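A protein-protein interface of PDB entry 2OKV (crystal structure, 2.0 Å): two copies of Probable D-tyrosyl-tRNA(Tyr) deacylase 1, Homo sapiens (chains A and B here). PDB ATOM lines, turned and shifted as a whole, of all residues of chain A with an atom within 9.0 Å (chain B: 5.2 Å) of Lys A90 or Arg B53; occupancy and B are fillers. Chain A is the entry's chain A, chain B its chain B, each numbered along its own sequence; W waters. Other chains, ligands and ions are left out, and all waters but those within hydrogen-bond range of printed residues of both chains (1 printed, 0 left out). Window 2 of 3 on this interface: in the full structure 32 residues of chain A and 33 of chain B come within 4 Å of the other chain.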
ATOM      1  N   THR A  81      23.761  -0.572  -3.220  1.00  0.00           N
ATOM      2  CA  THR A  81      22.809   0.256  -2.473  1.00  0.00           C
ATOM      3  C   THR A  81      23.313   1.657  -2.069  1.00  0.00           C
ATOM      4  O   THR A  81      22.555   2.446  -1.491  1.00  0.00           O
ATOM      5  CB  THR A  81      22.293  -0.489  -1.234  1.00  0.00           C
ATOM      6  OG1 THR A  81      23.400  -0.845  -0.411  1.00  0.00           O
ATOM      7  CG2 THR A  81      21.549  -1.764  -1.650  1.00  0.00           C
ATOM      8  N   GLN A  83      23.807   4.418  -3.703  1.00  0.00           N
ATOM      9  CA  GLN A  83      23.283   5.593  -4.416  1.00  0.00           C
ATOM     10  C   GLN A  83      22.295   6.421  -3.558  1.00  0.00           C
ATOM     11  O   GLN A  83      21.753   5.932  -2.559  1.00  0.00           O
ATOM     12  CB  GLN A  83      22.673   5.172  -5.762  1.00  0.00           C
ATOM     13  CG  GLN A  83      23.609   4.265  -6.618  1.00  0.00           C
ATOM     14  CD  GLN A  83      24.819   5.000  -7.222  1.00  0.00           C
ATOM     15  OE1 GLN A  83      25.892   4.415  -7.403  1.00  0.00           O
ATOM     16  NE2 GLN A  83      24.644   6.284  -7.537  1.00  0.00           N
ATOM     17  N   CYS A  84      22.081   7.678  -3.942  1.00  0.00           N
ATOM     18  CA  CYS A  84      21.258   8.592  -3.149  1.00  0.00           C
ATOM     19  C   CYS A  84      19.803   8.150  -3.045  1.00  0.00           C
ATOM     20  O   CYS A  84      19.195   7.718  -4.038  1.00  0.00           O
ATOM     21  CB  CYS A  84      21.336  10.018  -3.705  1.00  0.00           C
ATOM     22  SG  CYS A  84      22.931  10.807  -3.409  1.00  0.00           S
ATOM     23  N   VAL A  85      19.262   8.258  -1.830  1.00  0.00           N
ATOM     24  CA  VAL A  85      17.858   7.961  -1.559  1.00  0.00           C
ATOM     25  C   VAL A  85      16.954   9.044  -2.160  1.00  0.00           C
ATOM     26  O   VAL A  85      15.965   8.725  -2.828  1.00  0.00           O
ATOM     27  CB  VAL A  85      17.623   7.815  -0.054  1.00  0.00           C
ATOM     28  N   LEU A  86      17.297  10.314  -1.927  1.00  0.00           N
ATOM     29  CA  LEU A  86      16.619  11.451  -2.566  1.00  0.00           C
ATOM     30  C   LEU A  86      15.137  11.581  -2.262  1.00  0.00           C
ATOM     31  O   LEU A  86      14.725  12.423  -1.459  1.00  0.00           O
ATOM     32  N   LYS A  87      14.334  10.757  -2.932  1.00  0.00           N
ATOM     33  CA  LYS A  87      12.895  10.664  -2.664  1.00  0.00           C
ATOM     34  C   LYS A  87      12.532   9.252  -2.189  1.00  0.00           C
ATOM     35  O   LYS A  87      13.257   8.282  -2.466  1.00  0.00           O
ATOM     36  CB  LYS A  87      12.073  11.056  -3.896  1.00  0.00           C
ATOM     37  CG  LYS A  87      12.017  12.562  -4.158  1.00  0.00           C
ATOM     38  CD  LYS A  87      10.901  12.938  -5.141  1.00  0.00           C
ATOM     39  CE  LYS A  87      11.263  12.575  -6.583  1.00  0.00           C
ATOM     40  NZ  LYS A  87      10.183  12.918  -7.552  1.00  0.00           N
ATOM     41  N   GLY A  88      11.419   9.149  -1.461  1.00  0.00           N
ATOM     42  CA  GLY A  88      11.018   7.888  -0.841  1.00  0.00           C
ATOM     43  C   GLY A  88      11.977   7.435   0.258  1.00  0.00           C
ATOM     44  O   GLY A  88      12.955   8.123   0.582  1.00  0.00           O
ATOM     45  N   ASN A  89      11.699   6.260   0.817  1.00  0.00           N
ATOM     46  CA  ASN A  89      12.414   5.762   1.983  1.00  0.00           C
ATOM     47  C   ASN A  89      12.960   4.360   1.766  1.00  0.00           C
ATOM     48  O   ASN A  89      12.923   3.531   2.660  1.00  0.00           O
ATOM     49  CB  ASN A  89      11.490   5.779   3.201  1.00  0.00           C
ATOM     50  CG  ASN A  89      11.000   7.163   3.539  1.00  0.00           C
ATOM     51  OD1 ASN A  89      11.725   7.968   4.129  1.00  0.00           O
ATOM     52  ND2 ASN A  89       9.762   7.451   3.172  1.00  0.00           N
ATOM     53  N   LYS A  90      13.466   4.108   0.566  1.00  0.00           N
ATOM     54  CA  LYS A  90      14.063   2.819   0.215  1.00  0.00           C
ATOM     55  C   LYS A  90      15.323   3.059  -0.604  1.00  0.00           C
ATOM     56  O   LYS A  90      15.532   4.171  -1.093  1.00  0.00           O
ATOM     57  CB  LYS A  90      13.063   1.948  -0.565  1.00  0.00           C
ATOM     58  CG  LYS A  90      12.220   2.681  -1.603  1.00  0.00           C
ATOM     59  CD  LYS A  90      11.505   1.709  -2.548  1.00  0.00           C
ATOM     60  CE  LYS A  90      10.323   1.000  -1.895  1.00  0.00           C
ATOM     61  NZ  LYS A  90       9.015   1.640  -2.209  1.00  0.00           N
ATOM     62  N   PRO A  91      16.183   2.035  -0.747  1.00  0.00           N
ATOM     63  CA  PRO A  91      17.338   2.192  -1.633  1.00  0.00           C
ATOM     64  C   PRO A  91      16.919   2.550  -3.061  1.00  0.00           C
ATOM     65  O   PRO A  91      15.846   2.128  -3.518  1.00  0.00           O
ATOM     66  CB  PRO A  91      17.996   0.813  -1.593  1.00  0.00           C
ATOM     67  CG  PRO A  91      17.582   0.239  -0.299  1.00  0.00           C
ATOM     68  CD  PRO A  91      16.175   0.711  -0.101  1.00  0.00           C
ATOM     69  N   ASP A  92      17.741   3.358  -3.732  1.00  0.00           N
ATOM     70  CA  ASP A  92      17.458   3.793  -5.103  1.00  0.00           C
ATOM     71  C   ASP A  92      18.481   3.195  -6.054  1.00  0.00           C
ATOM     72  O   ASP A  92      19.689   3.392  -5.907  1.00  0.00           O
ATOM     73  CB  ASP A  92      17.455   5.316  -5.223  1.00  0.00           C
ATOM     74  CG  ASP A  92      16.817   5.801  -6.517  1.00  0.00           C
ATOM     75  OD1 ASP A  92      16.318   6.947  -6.528  1.00  0.00           O
ATOM     76  OD2 ASP A  92      16.796   5.045  -7.520  1.00  0.00           O
ATOM     77  N   PHE A  93      17.981   2.472  -7.040  1.00  0.00           N
ATOM     78  CA  PHE A  93      18.852   1.676  -7.879  1.00  0.00           C
ATOM     79  C   PHE A  93      18.967   2.178  -9.306  1.00  0.00           C
ATOM     80  O   PHE A  93      19.825   1.704 -10.048  1.00  0.00           O
ATOM     81  CB  PHE A  93      18.412   0.214  -7.843  1.00  0.00           C
ATOM     82  CG  PHE A  93      18.337  -0.349  -6.460  1.00  0.00           C
ATOM     83  CD1 PHE A  93      17.238  -1.086  -6.060  1.00  0.00           C
ATOM     84  CD2 PHE A  93      19.353  -0.112  -5.546  1.00  0.00           C
ATOM     85  CE1 PHE A  93      17.161  -1.603  -4.783  1.00  0.00           C
ATOM     86  CE2 PHE A  93      19.285  -0.632  -4.263  1.00  0.00           C
ATOM     87  CZ  PHE A  93      18.178  -1.385  -3.889  1.00  0.00           C
ATOM     88  N   ASN B  51      12.168   5.632   9.297  1.00  0.00           N
ATOM     89  CA  ASN B  51      11.285   5.285   8.183  1.00  0.00           C
ATOM     90  C   ASN B  51      11.967   4.601   6.979  1.00  0.00           C
ATOM     91  O   ASN B  51      11.300   4.186   6.017  1.00  0.00           O
ATOM     92  CB  ASN B  51      10.471   6.523   7.812  1.00  0.00           C
ATOM     93  CG  ASN B  51       9.526   6.957   8.959  1.00  0.00           C
ATOM     94  OD1 ASN B  51       8.445   6.367   9.144  1.00  0.00           O
ATOM     95  ND2 ASN B  51       9.939   7.977   9.752  1.00  0.00           N
ATOM     96  N   LEU B  52      13.291   4.444   7.057  1.00  0.00           N
ATOM     97  CA  LEU B  52      14.082   3.834   5.992  1.00  0.00           C
ATOM     98  C   LEU B  52      13.721   2.353   5.785  1.00  0.00           C
ATOM     99  O   LEU B  52      13.940   1.516   6.673  1.00  0.00           O
ATOM    100  CB  LEU B  52      15.568   3.944   6.334  1.00  0.00           C
ATOM    101  CG  LEU B  52      16.699   3.978   5.286  1.00  0.00           C
ATOM    102  CD1 LEU B  52      17.874   3.137   5.753  1.00  0.00           C
ATOM    103  CD2 LEU B  52      16.294   3.653   3.881  1.00  0.00           C
ATOM    104  N   ARG B  53      13.215   2.046   4.598  1.00  0.00           N
ATOM    105  CA  ARG B  53      12.721   0.706   4.255  1.00  0.00           C
ATOM    106  C   ARG B  53      13.845  -0.208   3.760  1.00  0.00           C
ATOM    107  O   ARG B  53      14.089  -0.333   2.553  1.00  0.00           O
ATOM    108  CB  ARG B  53      11.643   0.788   3.174  1.00  0.00           C
ATOM    109  CG  ARG B  53      10.300   1.400   3.580  1.00  0.00           C
ATOM    110  CD  ARG B  53       9.451   1.680   2.294  1.00  0.00           C
ATOM    111  NE  ARG B  53       8.062   1.265   2.433  1.00  0.00           N
ATOM    112  CZ  ARG B  53       7.402   0.486   1.568  1.00  0.00           C
ATOM    113  NH1 ARG B  53       7.991   0.017   0.464  1.00  0.00           N
ATOM    114  NH2 ARG B  53       6.141   0.164   1.810  1.00  0.00           N
ATOM    115  N   VAL B  54      14.490  -0.872   4.703  1.00  0.00           N
ATOM    116  CA  VAL B  54      15.645  -1.692   4.414  1.00  0.00           C
ATOM    117  C   VAL B  54      15.357  -3.190   4.657  1.00  0.00           C
ATOM    118  O   VAL B  54      16.187  -4.061   4.369  1.00  0.00           O
ATOM    119  CB  VAL B  54      16.821  -1.120   5.243  1.00  0.00           C
ATOM    120  CG1 VAL B  54      17.340  -2.083   6.284  1.00  0.00           C
ATOM    121  CG2 VAL B  54      17.871  -0.513   4.356  1.00  0.00           C
ATOM    122  N   PHE B  55      14.158  -3.477   5.164  1.00  0.00           N
ATOM    123  CA  PHE B  55      13.769  -4.847   5.521  1.00  0.00           C
ATOM    124  C   PHE B  55      12.711  -5.442   4.599  1.00  0.00           C
ATOM    125  O   PHE B  55      11.964  -4.710   3.943  1.00  0.00           O
ATOM    126  CB  PHE B  55      13.312  -4.902   6.986  1.00  0.00           C
ATOM    127  CG  PHE B  55      14.379  -4.468   7.954  1.00  0.00           C
ATOM    128  CD1 PHE B  55      14.375  -3.180   8.493  1.00  0.00           C
ATOM    129  CD2 PHE B  55      15.413  -5.340   8.303  1.00  0.00           C
ATOM    130  CE1 PHE B  55      15.399  -2.762   9.367  1.00  0.00           C
ATOM    131  CE2 PHE B  55      16.437  -4.935   9.188  1.00  0.00           C
ATOM    132  CZ  PHE B  55      16.426  -3.637   9.708  1.00  0.00           C
ATOM    133  N   LYS B  61       9.416  -9.725  -0.199  1.00  0.00           N
ATOM    134  CA  LYS B  61       9.604  -8.515  -1.006  1.00  0.00           C
ATOM    135  C   LYS B  61      10.618  -7.595  -0.313  1.00  0.00           C
ATOM    136  O   LYS B  61      10.480  -7.299   0.872  1.00  0.00           O
ATOM    137  CB  LYS B  61       8.279  -7.775  -1.149  1.00  0.00           C
ATOM    138  CG  LYS B  61       8.228  -6.805  -2.460  1.00  0.00           C
ATOM    139  CD  LYS B  61       7.608  -5.402  -2.123  1.00  0.00           C
ATOM    140  CE  LYS B  61       6.239  -5.592  -1.364  1.00  0.00           C
ATOM    141  NZ  LYS B  61       5.842  -4.370  -0.534  1.00  0.00           N
ATOM    142  N   TRP B  63      12.837  -4.113   0.576  1.00  0.00           N
ATOM    143  CA  TRP B  63      12.617  -2.669   0.733  1.00  0.00           C
ATOM    144  C   TRP B  63      11.181  -2.308   1.081  1.00  0.00           C
ATOM    145  O   TRP B  63      10.639  -1.315   0.572  1.00  0.00           O
ATOM    146  CB  TRP B  63      13.063  -1.915  -0.539  1.00  0.00           C
ATOM    147  CG  TRP B  63      14.315  -2.495  -1.189  1.00  0.00           C
ATOM    148  CD1 TRP B  63      14.468  -2.876  -2.489  1.00  0.00           C
ATOM    149  CD2 TRP B  63      15.566  -2.777  -0.539  1.00  0.00           C
ATOM    150  NE1 TRP B  63      15.739  -3.378  -2.694  1.00  0.00           N
ATOM    151  CE2 TRP B  63      16.433  -3.321  -1.514  1.00  0.00           C
ATOM    152  CE3 TRP B  63      16.033  -2.626   0.776  1.00  0.00           C
ATOM    153  CZ2 TRP B  63      17.746  -3.705  -1.219  1.00  0.00           C
ATOM    154  CZ3 TRP B  63      17.344  -3.005   1.071  1.00  0.00           C
ATOM    155  CH2 TRP B  63      18.182  -3.536   0.078  1.00  0.00           C
ATOM    156  N   SER B  64      10.538  -3.112   1.921  1.00  0.00           N
ATOM    157  CA  SER B  64       9.112  -2.865   2.204  1.00  0.00           C
ATOM    158  C   SER B  64       8.805  -2.519   3.659  1.00  0.00           C
ATOM    159  O   SER B  64       7.705  -2.085   3.971  1.00  0.00           O
ATOM    160  CB  SER B  64       8.217  -4.016   1.712  1.00  0.00           C
ATOM    161  OG  SER B  64       8.666  -5.275   2.179  1.00  0.00           O
ATOM    162  N   LYS B  65       9.773  -2.711   4.548  1.00  0.00           N
ATOM    163  CA  LYS B  65       9.542  -2.454   5.964  1.00  0.00           C
ATOM    164  C   LYS B  65      10.705  -1.681   6.576  1.00  0.00           C
ATOM    165  O   LYS B  65      11.879  -1.955   6.279  1.00  0.00           O
ATOM    166  CB  LYS B  65       9.325  -3.768   6.720  1.00  0.00           C
ATOM    167  CG  LYS B  65       8.162  -4.631   6.216  1.00  0.00           C
ATOM    168  CD  LYS B  65       6.865  -4.355   6.934  1.00  0.00           C
ATOM    169  CE  LYS B  65       5.743  -5.227   6.370  1.00  0.00           C
ATOM    170  NZ  LYS B  65       4.530  -5.177   7.235  1.00  0.00           N
ATOM    171  N   SER B  66      10.384  -0.719   7.436  1.00  0.00           N
ATOM    172  CA  SER B  66      11.424  -0.015   8.210  1.00  0.00           C
ATOM    173  C   SER B  66      11.767  -0.761   9.501  1.00  0.00           C
ATOM    174  O   SER B  66      11.084  -1.710   9.875  1.00  0.00           O
ATOM    175  CB  SER B  66      10.936   1.375   8.562  1.00  0.00           C
ATOM    176  OG  SER B  66       9.825   1.294   9.445  1.00  0.00           O
HETATM  177  O   HOH W   1      14.148   7.114   5.032  1.00  0.00           O
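N of Arg B53 is in hydrogen-bond range of O of Asn A89 (2.5 Å). NH1 of Arg B53 lies close to NZ of Lys A90 (3.3 Å).
O of Ser B64 sits at hydrogen-bond distance from NH2 of Arg B53. O of Trp B63 sits at hydrogen-bond distance from NH1 of Arg B53, 3.0 Å away.
Asn A89 touches Asn B51. Asn A89 touches Leu B52. Lys A90 touches Trp B63 (CE to O, 3.4 Å). Pro A91 touches Arg B53 (CD to O, 3.5 Å). Pro A91 touches Trp B63 (CG to CE3, 3.4 Å). Phe A93 touches Trp B63.
Lys A90 touches two residues of chain B. Leu B52 touches just one residue of chain A: Asn A89. No residue of chain A comes within 4 Å of Val B54. Of the printed residues of chain A, Asn B51 touches Asn A89. Of the printed residues of chain B, Asn A89 touches Asn B51 (3.2 Å), Leu B52 (3.4 Å) and Arg B53 (2.5 Å). Of the printed residues of chain B, Pro A91 touches Arg B53 (3.5 Å) and Trp B63 (3.4 Å). Ser B66 touches none of the printed residues of chain A. The nearest residue of chain B that does not touch Lys A90 is Leu B52 (4.4 Å). The nearest residue of chain A that does not touch Arg B53 is Gly A88 (6.6 Å).
Printed residues of chain B that touch a printed residue of chain A: Asn B51, Leu B52, Arg B53 and Trp B63. Along chain B the printed residues that touch a printed residue of chain A span positions 51 to 63. Of the 12 printed residues of chain A, 4 touch a printed residue of chain B. Printed residues of chain A that touch a printed residue of chain B: Asn A89, Lys A90, Pro A91 and Phe A93. Hydrophobic or aromatic side chains of chain A that line the printed part of chain B: Pro A91 and Phe A93.
No position is printed for both chains. Of the 8 pairs that touch across the chains among the printed residues, none has its exchanged pair printed and touching as well.
Water W1 lies within hydrogen-bond range of the side-chain amide oxygen (OD1) of Asn A89 (2.7 Å) and the backbone NH (N) of Leu B52 (3.5 Å).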
